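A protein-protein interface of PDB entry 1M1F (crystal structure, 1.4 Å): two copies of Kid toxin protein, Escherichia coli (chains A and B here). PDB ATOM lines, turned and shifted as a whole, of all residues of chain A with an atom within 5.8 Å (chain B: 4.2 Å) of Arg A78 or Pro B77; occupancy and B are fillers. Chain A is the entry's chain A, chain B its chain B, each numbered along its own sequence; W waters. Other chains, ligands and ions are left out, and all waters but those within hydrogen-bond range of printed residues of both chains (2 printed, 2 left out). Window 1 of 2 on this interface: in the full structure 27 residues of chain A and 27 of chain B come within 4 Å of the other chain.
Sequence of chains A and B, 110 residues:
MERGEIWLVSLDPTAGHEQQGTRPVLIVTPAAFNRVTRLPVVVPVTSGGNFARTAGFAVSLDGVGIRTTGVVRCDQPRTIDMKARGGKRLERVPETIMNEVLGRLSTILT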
ATOM      1  N   LEU A  11      -4.965 -19.421   5.976  1.00  0.00           N
ATOM      2  CA  LEU A  11      -6.349 -19.472   5.503  1.00  0.00           C
ATOM      3  C   LEU A  11      -6.479 -20.212   4.174  1.00  0.00           C
ATOM      4  O   LEU A  11      -7.584 -20.370   3.654  1.00  0.00           O
ATOM      5  CB  LEU A  11      -6.870 -18.048   5.323  1.00  0.00           C
ATOM      6  CG  LEU A  11      -6.964 -17.199   6.593  1.00  0.00           C
ATOM      7  CD1 LEU A  11      -7.414 -15.779   6.280  1.00  0.00           C
ATOM      8  CD2 LEU A  11      -7.906 -17.860   7.583  1.00  0.00           C
ATOM      9  N   ASP A  12      -5.359 -20.673   3.629  1.00  0.00           N
ATOM     10  CA  ASP A  12      -5.358 -21.335   2.327  1.00  0.00           C
ATOM     11  C   ASP A  12      -5.758 -22.804   2.461  1.00  0.00           C
ATOM     12  O   ASP A  12      -5.652 -23.380   3.539  1.00  0.00           O
ATOM     13  CB  ASP A  12      -3.969 -21.223   1.685  1.00  0.00           C
ATOM     14  CG  ASP A  12      -3.566 -19.787   1.379  1.00  0.00           C
ATOM     15  OD1 ASP A  12      -4.408 -18.967   0.940  1.00  0.00           O
ATOM     16  OD2 ASP A  12      -2.389 -19.380   1.545  1.00  0.00           O
ATOM     17  N   PRO A  13      -6.234 -23.428   1.378  1.00  0.00           N
ATOM     18  CA  PRO A  13      -6.457 -22.791   0.075  1.00  0.00           C
ATOM     19  C   PRO A  13      -7.808 -22.101  -0.012  1.00  0.00           C
ATOM     20  O   PRO A  13      -8.704 -22.402   0.775  1.00  0.00           O
ATOM     21  CB  PRO A  13      -6.454 -23.971  -0.904  1.00  0.00           C
ATOM     22  CG  PRO A  13      -6.640 -25.185  -0.104  1.00  0.00           C
ATOM     23  CD  PRO A  13      -6.536 -24.863   1.349  1.00  0.00           C
ATOM     24  N   THR A  14      -7.951 -21.210  -0.989  1.00  0.00           N
ATOM     25  CA  THR A  14      -9.172 -20.420  -1.153  1.00  0.00           C
ATOM     26  C   THR A  14      -9.579 -20.345  -2.608  1.00  0.00           C
ATOM     27  O   THR A  14      -8.831 -20.761  -3.502  1.00  0.00           O
ATOM     28  CB  THR A  14      -8.963 -18.981  -0.667  1.00  0.00           C
ATOM     29  OG1 THR A  14      -7.989 -18.339  -1.500  1.00  0.00           O
ATOM     30  CG2 THR A  14      -8.384 -18.939   0.743  1.00  0.00           C
ATOM     31  N   GLN A  19     -10.397 -14.070   1.044  1.00  0.00           N
ATOM     32  CA  GLN A  19      -9.160 -13.621   1.657  1.00  0.00           C
ATOM     33  C   GLN A  19      -8.159 -14.773   1.680  1.00  0.00           C
ATOM     34  O   GLN A  19      -8.472 -15.866   2.146  1.00  0.00           O
ATOM     35  CB  GLN A  19      -9.427 -13.115   3.071  1.00  0.00           C
ATOM     36  CG  GLN A  19      -8.220 -12.445   3.700  1.00  0.00           C
ATOM     37  CD  GLN A  19      -7.816 -11.171   2.981  1.00  0.00           C
ATOM     38  OE1 GLN A  19      -6.675 -11.040   2.534  1.00  0.00           O
ATOM     39  NE2 GLN A  19      -8.746 -10.240   2.858  1.00  0.00           N
ATOM     40  N   PRO A  40     -13.397 -22.219  16.166  1.00  0.00           N
ATOM     41  CA  PRO A  40     -13.661 -20.802  16.416  1.00  0.00           C
ATOM     42  C   PRO A  40     -14.067 -20.064  15.148  1.00  0.00           C
ATOM     43  O   PRO A  40     -13.661 -20.424  14.045  1.00  0.00           O
ATOM     44  CB  PRO A  40     -12.303 -20.277  16.896  1.00  0.00           C
ATOM     45  CG  PRO A  40     -11.328 -21.229  16.293  1.00  0.00           C
ATOM     46  CD  PRO A  40     -11.989 -22.566  16.431  1.00  0.00           C
ATOM     47  N   VAL A  41     -14.870 -19.025  15.329  1.00  0.00           N
ATOM     48  CA  VAL A  41     -15.155 -18.091  14.262  1.00  0.00           C
ATOM     49  C   VAL A  41     -14.149 -16.942  14.397  1.00  0.00           C
ATOM     50  O   VAL A  41     -13.944 -16.406  15.489  1.00  0.00           O
ATOM     51  CB  VAL A  41     -16.605 -17.547  14.328  1.00  0.00           C
ATOM     52  CG1 VAL A  41     -16.839 -16.575  13.188  1.00  0.00           C
ATOM     53  CG2 VAL A  41     -17.598 -18.695  14.282  1.00  0.00           C
ATOM     54  N   VAL A  42     -13.524 -16.586  13.282  1.00  0.00           N
ATOM     55  CA  VAL A  42     -12.506 -15.550  13.238  1.00  0.00           C
ATOM     56  C   VAL A  42     -12.776 -14.565  12.111  1.00  0.00           C
ATOM     57  O   VAL A  42     -13.523 -14.856  11.176  1.00  0.00           O
ATOM     58  CB  VAL A  42     -11.075 -16.163  13.027  1.00  0.00           C
ATOM     59  CG1 VAL A  42     -10.831 -17.292  14.000  1.00  0.00           C
ATOM     60  CG2 VAL A  42     -10.881 -16.646  11.596  1.00  0.00           C
ATOM     61  N   VAL A  43     -12.172 -13.383  12.218  1.00  0.00           N
ATOM     62  CA  VAL A  43     -12.167 -12.417  11.119  1.00  0.00           C
ATOM     63  C   VAL A  43     -10.705 -12.069  10.813  1.00  0.00           C
ATOM     64  O   VAL A  43      -9.879 -11.944  11.727  1.00  0.00           O
ATOM     65  CB  VAL A  43     -13.005 -11.159  11.407  1.00  0.00           C
ATOM     66  CG1 VAL A  43     -14.480 -11.476  11.263  1.00  0.00           C
ATOM     67  CG2 VAL A  43     -12.705 -10.567  12.779  1.00  0.00           C
ATOM     68  N   GLN A  76     -15.638 -10.516   6.686  1.00  0.00           N
ATOM     69  CA  GLN A  76     -15.226 -11.842   6.222  1.00  0.00           C
ATOM     70  C   GLN A  76     -15.049 -12.862   7.341  1.00  0.00           C
ATOM     71  O   GLN A  76     -13.992 -13.490   7.463  1.00  0.00           O
ATOM     72  CB  GLN A  76     -13.938 -11.766   5.379  1.00  0.00           C
ATOM     73  CG  GLN A  76     -14.092 -10.981   4.061  1.00  0.00           C
ATOM     74  CD  GLN A  76     -13.079 -11.356   2.932  1.00  0.00           C
ATOM     75  OE1 GLN A  76     -12.530 -10.454   2.287  1.00  0.00           O
ATOM     76  NE2 GLN A  76     -12.897 -12.660   2.653  1.00  0.00           N
ATOM     77  N   PRO A  77     -16.077 -13.096   8.147  1.00  0.00           N
ATOM     78  CA  PRO A  77     -15.950 -14.113   9.190  1.00  0.00           C
ATOM     79  C   PRO A  77     -15.802 -15.515   8.596  1.00  0.00           C
ATOM     80  O   PRO A  77     -16.380 -15.821   7.543  1.00  0.00           O
ATOM     81  CB  PRO A  77     -17.263 -13.986   9.950  1.00  0.00           C
ATOM     82  CG  PRO A  77     -18.222 -13.462   8.928  1.00  0.00           C
ATOM     83  CD  PRO A  77     -17.422 -12.472   8.146  1.00  0.00           C
ATOM     84  N   ARG A  78     -15.065 -16.363   9.296  1.00  0.00           N
ATOM     85  CA  ARG A  78     -14.863 -17.727   8.867  1.00  0.00           C
ATOM     86  C   ARG A  78     -14.678 -18.631  10.062  1.00  0.00           C
ATOM     87  O   ARG A  78     -13.954 -18.294  11.001  1.00  0.00           O
ATOM     88  CB  ARG A  78     -13.600 -17.779   8.039  1.00  0.00           C
ATOM     89  CG  ARG A  78     -13.372 -19.001   7.341  1.00  0.00           C
ATOM     90  CD  ARG A  78     -12.425 -18.802   6.197  1.00  0.00           C
ATOM     91  NE  ARG A  78     -11.911 -20.091   5.890  1.00  0.00           N
ATOM     92  CZ  ARG A  78     -10.829 -20.326   5.189  1.00  0.00           C
ATOM     93  NH1 ARG A  78     -10.130 -19.340   4.642  1.00  0.00           N
ATOM     94  NH2 ARG A  78     -10.474 -21.576   5.031  1.00  0.00           N
ATOM     95  N   THR A  79     -15.323 -19.787  10.017  1.00  0.00           N
ATOM     96  CA  THR A  79     -15.160 -20.814  11.024  1.00  0.00           C
ATOM     97  C   THR A  79     -13.972 -21.666  10.607  1.00  0.00           C
ATOM     98  O   THR A  79     -13.950 -22.187   9.493  1.00  0.00           O
ATOM     99  CB  THR A  79     -16.431 -21.660  11.069  1.00  0.00           C
ATOM    100  OG1 THR A  79     -17.533 -20.838  11.492  1.00  0.00           O
ATOM    101  CG2 THR A  79     -16.316 -22.766  12.085  1.00  0.00           C
ATOM    102  N   ILE A  80     -12.978 -21.795  11.477  1.00  0.00           N
ATOM    103  CA  ILE A  80     -11.791 -22.582  11.130  1.00  0.00           C
ATOM    104  C   ILE A  80     -11.376 -23.527  12.239  1.00  0.00           C
ATOM    105  O   ILE A  80     -11.614 -23.283  13.420  1.00  0.00           O
ATOM    106  CB  ILE A  80     -10.582 -21.662  10.738  1.00  0.00           C
ATOM    107  CG1 ILE A  80     -10.163 -20.751  11.897  1.00  0.00           C
ATOM    108  CG2 ILE A  80     -10.908 -20.841   9.485  1.00  0.00           C
ATOM    109  CD1 ILE A  80      -8.823 -20.040  11.659  1.00  0.00           C
ATOM    110  N   ARG A  85      -5.158 -26.367  11.504  1.00  0.00           N
ATOM    111  CA  ARG A  85      -4.411 -25.462  10.654  1.00  0.00           C
ATOM    112  C   ARG A  85      -3.064 -25.026  11.255  1.00  0.00           C
ATOM    113  O   ARG A  85      -2.283 -24.389  10.575  1.00  0.00           O
ATOM    114  CB  ARG A  85      -5.252 -24.224  10.332  1.00  0.00           C
ATOM    115  CG  ARG A  85      -6.368 -24.476   9.327  1.00  0.00           C
ATOM    116  CD  ARG A  85      -7.245 -23.251   9.009  1.00  0.00           C
ATOM    117  NE  ARG A  85      -8.250 -23.625   8.022  1.00  0.00           N
ATOM    118  CZ  ARG A  85      -8.082 -23.585   6.707  1.00  0.00           C
ATOM    119  NH1 ARG A  85      -6.973 -23.100   6.168  1.00  0.00           N
ATOM    120  NH2 ARG A  85      -9.041 -24.030   5.916  1.00  0.00           N
ATOM    121  N   LEU A 109     -24.864 -10.446  10.889  1.00  0.00           N
ATOM    122  CA  LEU A 109     -25.136 -11.794  11.394  1.00  0.00           C
ATOM    123  C   LEU A 109     -26.329 -11.899  12.356  1.00  0.00           C
ATOM    124  O   LEU A 109     -26.418 -12.868  13.125  1.00  0.00           O
ATOM    125  CB  LEU A 109     -23.885 -12.328  12.086  1.00  0.00           C
ATOM    126  CG  LEU A 109     -22.604 -12.342  11.253  1.00  0.00           C
ATOM    127  CD1 LEU A 109     -21.542 -13.028  12.067  1.00  0.00           C
ATOM    128  CD2 LEU A 109     -22.755 -13.003   9.884  1.00  0.00           C
ATOM    129  N   VAL B  41     -21.769 -14.393   3.379  1.00  0.00           N
ATOM    130  CA  VAL B  41     -21.549 -15.242   4.536  1.00  0.00           C
ATOM    131  C   VAL B  41     -22.670 -16.284   4.507  1.00  0.00           C
ATOM    132  O   VAL B  41     -23.854 -15.934   4.315  1.00  0.00           O
ATOM    133  CB  VAL B  41     -21.608 -14.458   5.850  1.00  0.00           C
ATOM    134  CG1 VAL B  41     -21.371 -15.387   7.033  1.00  0.00           C
ATOM    135  CG2 VAL B  41     -20.597 -13.332   5.832  1.00  0.00           C
ATOM    136  N   VAL B  42     -22.290 -17.550   4.661  1.00  0.00           N
ATOM    137  CA  VAL B  42     -23.225 -18.665   4.622  1.00  0.00           C
ATOM    138  C   VAL B  42     -23.033 -19.568   5.829  1.00  0.00           C
ATOM    139  O   VAL B  42     -21.977 -19.550   6.480  1.00  0.00           O
ATOM    140  CB  VAL B  42     -23.038 -19.513   3.339  1.00  0.00           C
ATOM    141  CG1 VAL B  42     -23.023 -18.621   2.117  1.00  0.00           C
ATOM    142  CG2 VAL B  42     -21.776 -20.367   3.397  1.00  0.00           C
ATOM    143  N   VAL B  43     -24.074 -20.329   6.153  1.00  0.00           N
ATOM    144  CA  VAL B  43     -23.966 -21.378   7.158  1.00  0.00           C
ATOM    145  C   VAL B  43     -24.339 -22.695   6.477  1.00  0.00           C
ATOM    146  O   VAL B  43     -25.263 -22.746   5.664  1.00  0.00           O
ATOM    147  CB  VAL B  43     -24.825 -21.118   8.410  1.00  0.00           C
ATOM    148  CG1 VAL B  43     -24.138 -20.070   9.307  1.00  0.00           C
ATOM    149  CG2 VAL B  43     -26.224 -20.681   8.038  1.00  0.00           C
ATOM    150  N   CYS B  74     -25.695 -23.184  12.619  1.00  0.00           N
ATOM    151  CA  CYS B  74     -25.618 -21.746  12.839  1.00  0.00           C
ATOM    152  C   CYS B  74     -24.329 -21.342  13.536  1.00  0.00           C
ATOM    153  O   CYS B  74     -24.023 -20.150  13.620  1.00  0.00           O
ATOM    154  CB  CYS B  74     -26.833 -21.272  13.635  1.00  0.00           C
ATOM    155  SG  CYS B  74     -28.393 -21.628  12.822  1.00  0.00           S
ATOM    156  N   ASP B  75     -23.594 -22.331  14.043  1.00  0.00           N
ATOM    157  CA  ASP B  75     -22.308 -22.108  14.688  1.00  0.00           C
ATOM    158  C   ASP B  75     -21.141 -22.106  13.700  1.00  0.00           C
ATOM    159  O   ASP B  75     -20.000 -21.868  14.108  1.00  0.00           O
ATOM    160  CB  ASP B  75     -22.051 -23.131  15.816  1.00  0.00           C
ATOM    161  CG  ASP B  75     -22.260 -24.574  15.407  1.00  0.00           C
ATOM    162  OD1 ASP B  75     -22.866 -24.858  14.364  1.00  0.00           O
ATOM    163  OD2 ASP B  75     -21.862 -25.515  16.144  1.00  0.00           O
ATOM    164  N   GLN B  76     -21.417 -22.291  12.409  1.00  0.00           N
ATOM    165  CA  GLN B  76     -20.341 -22.439  11.433  1.00  0.00           C
ATOM    166  C   GLN B  76     -20.403 -21.501  10.231  1.00  0.00           C
ATOM    167  O   GLN B  76     -20.299 -21.942   9.088  1.00  0.00           O
ATOM    168  CB  GLN B  76     -20.242 -23.901  10.979  1.00  0.00           C
ATOM    169  CG  GLN B  76     -19.968 -24.843  12.148  1.00  0.00           C
ATOM    170  CD  GLN B  76     -19.842 -26.294  11.758  1.00  0.00           C
ATOM    171  OE1 GLN B  76     -19.650 -26.617  10.592  1.00  0.00           O
ATOM    172  NE2 GLN B  76     -19.922 -27.180  12.750  1.00  0.00           N
ATOM    173  N   PRO B  77     -20.500 -20.201  10.467  1.00  0.00           N
ATOM    174  CA  PRO B  77     -20.533 -19.269   9.341  1.00  0.00           C
ATOM    175  C   PRO B  77     -19.207 -19.259   8.580  1.00  0.00           C
ATOM    176  O   PRO B  77     -18.126 -19.452   9.150  1.00  0.00           O
ATOM    177  CB  PRO B  77     -20.758 -17.923  10.018  1.00  0.00           C
ATOM    178  CG  PRO B  77     -20.131 -18.101  11.367  1.00  0.00           C
ATOM    179  CD  PRO B  77     -20.543 -19.493  11.761  1.00  0.00           C
ATOM    180  N   ARG B  78     -19.301 -19.001   7.289  1.00  0.00           N
ATOM    181  CA  ARG B  78     -18.137 -18.916   6.435  1.00  0.00           C
ATOM    182  C   ARG B  78     -18.409 -17.967   5.280  1.00  0.00           C
ATOM    183  O   ARG B  78     -19.449 -18.025   4.657  1.00  0.00           O
ATOM    184  CB  ARG B  78     -17.820 -20.306   5.870  1.00  0.00           C
ATOM    185  CG  ARG B  78     -16.524 -20.400   5.115  1.00  0.00           C
ATOM    186  CD  ARG B  78     -16.268 -21.754   4.509  1.00  0.00           C
ATOM    187  NE  ARG B  78     -15.107 -21.690   3.656  1.00  0.00           N
ATOM    188  CZ  ARG B  78     -14.748 -22.643   2.828  1.00  0.00           C
ATOM    189  NH1 ARG B  78     -15.430 -23.778   2.783  1.00  0.00           N
ATOM    190  NH2 ARG B  78     -13.685 -22.462   2.055  1.00  0.00           N
ATOM    191  N   LEU B 105     -27.358 -17.800  15.356  1.00  0.00           N
ATOM    192  CA  LEU B 105     -26.096 -17.278  14.859  1.00  0.00           C
ATOM    193  C   LEU B 105     -25.661 -16.039  15.644  1.00  0.00           C
ATOM    194  O   LEU B 105     -24.491 -15.905  16.014  1.00  0.00           O
ATOM    195  CB  LEU B 105     -26.216 -16.978  13.366  1.00  0.00           C
ATOM    196  CG  LEU B 105     -25.017 -16.283  12.734  1.00  0.00           C
ATOM    197  CD1 LEU B 105     -23.752 -17.101  12.831  1.00  0.00           C
ATOM    198  CD2 LEU B 105     -25.366 -15.997  11.282  1.00  0.00           C
HETATM  199  O   HOH W   1     -13.934 -19.168   3.395  1.00  0.00           O
HETATM  200  O   HOH W   2     -11.328 -23.683   0.098  1.00  0.00           O
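The backbone carbonyl oxygen of Pro B77 sits at hydrogen-bond distance from the side-chain hydroxyl of Thr A79 (2.8 Å).
NH1 of Arg A78 sits at hydrogen-bond distance from O of Leu A11 (2.9 Å). The backbone carbonyl oxygen of Val A42 lies within hydrogen-bond range of the backbone NH of Arg A78 (2.9 Å). The backbone carbonyl oxygen (O) of Val B42 is in hydrogen-bond range of the backbone NH (N) of Arg B78.
Among the printed residues, pairs that only touch across the chains: Thr A79 with Gln B76, Arg A78 with Pro B77, Leu A109 with Leu B105, Pro A77 with Arg B78, Thr A79 with Asp B75, Pro A77 with Val B41, Val A41 with Pro B77, Leu A109 with Val B41 and Val A41 with Asp B75.
Arg A78 touches just one residue of chain B: Pro B77 (3.7 Å). Of the printed residues of chain B, Thr A79 touches Asp B75 (3.7 Å), Gln B76 (3.2 Å) and Pro B77 (2.8 Å). Of the printed residues of chain A, Val B41 touches Pro A77 and Leu A109. Pro B77 touches just these residues of chain A: Val A41 (3.9 Å), Arg A78 (3.7 Å) and Thr A79 (2.8 Å). Of the printed residues of chain A, Arg B78 touches Pro A77. The nearest residue of chain A that does not touch Pro B77 is Pro A77 (4.3 Å).
Hydrophobic or aromatic side chains of chain B that line the printed part of chain A: Val B41, Pro B77 and Leu B105. Of the 16 printed residues of chain A, 5 touch a printed residue of chain B.
Val A41 touches Pro B77, and with the chains exchanged Pro A77 touches Val B41. Pro A77 touches Arg B78, and with the chains exchanged Arg A78 touches Pro B77. Positions printed for both chains: 41, 42, 43, 76, 77 and 78. Of the 10 pairs that touch across the chains among the printed residues, 4 have their exchanged pair printed and touching as well.
Water W1 lies within hydrogen-bond range of NE of Arg B78 and NE of Arg A78. Water W2 bridges O of Pro A13 (3.0 Å) and NH2 of Arg B78 (3.3 Å).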
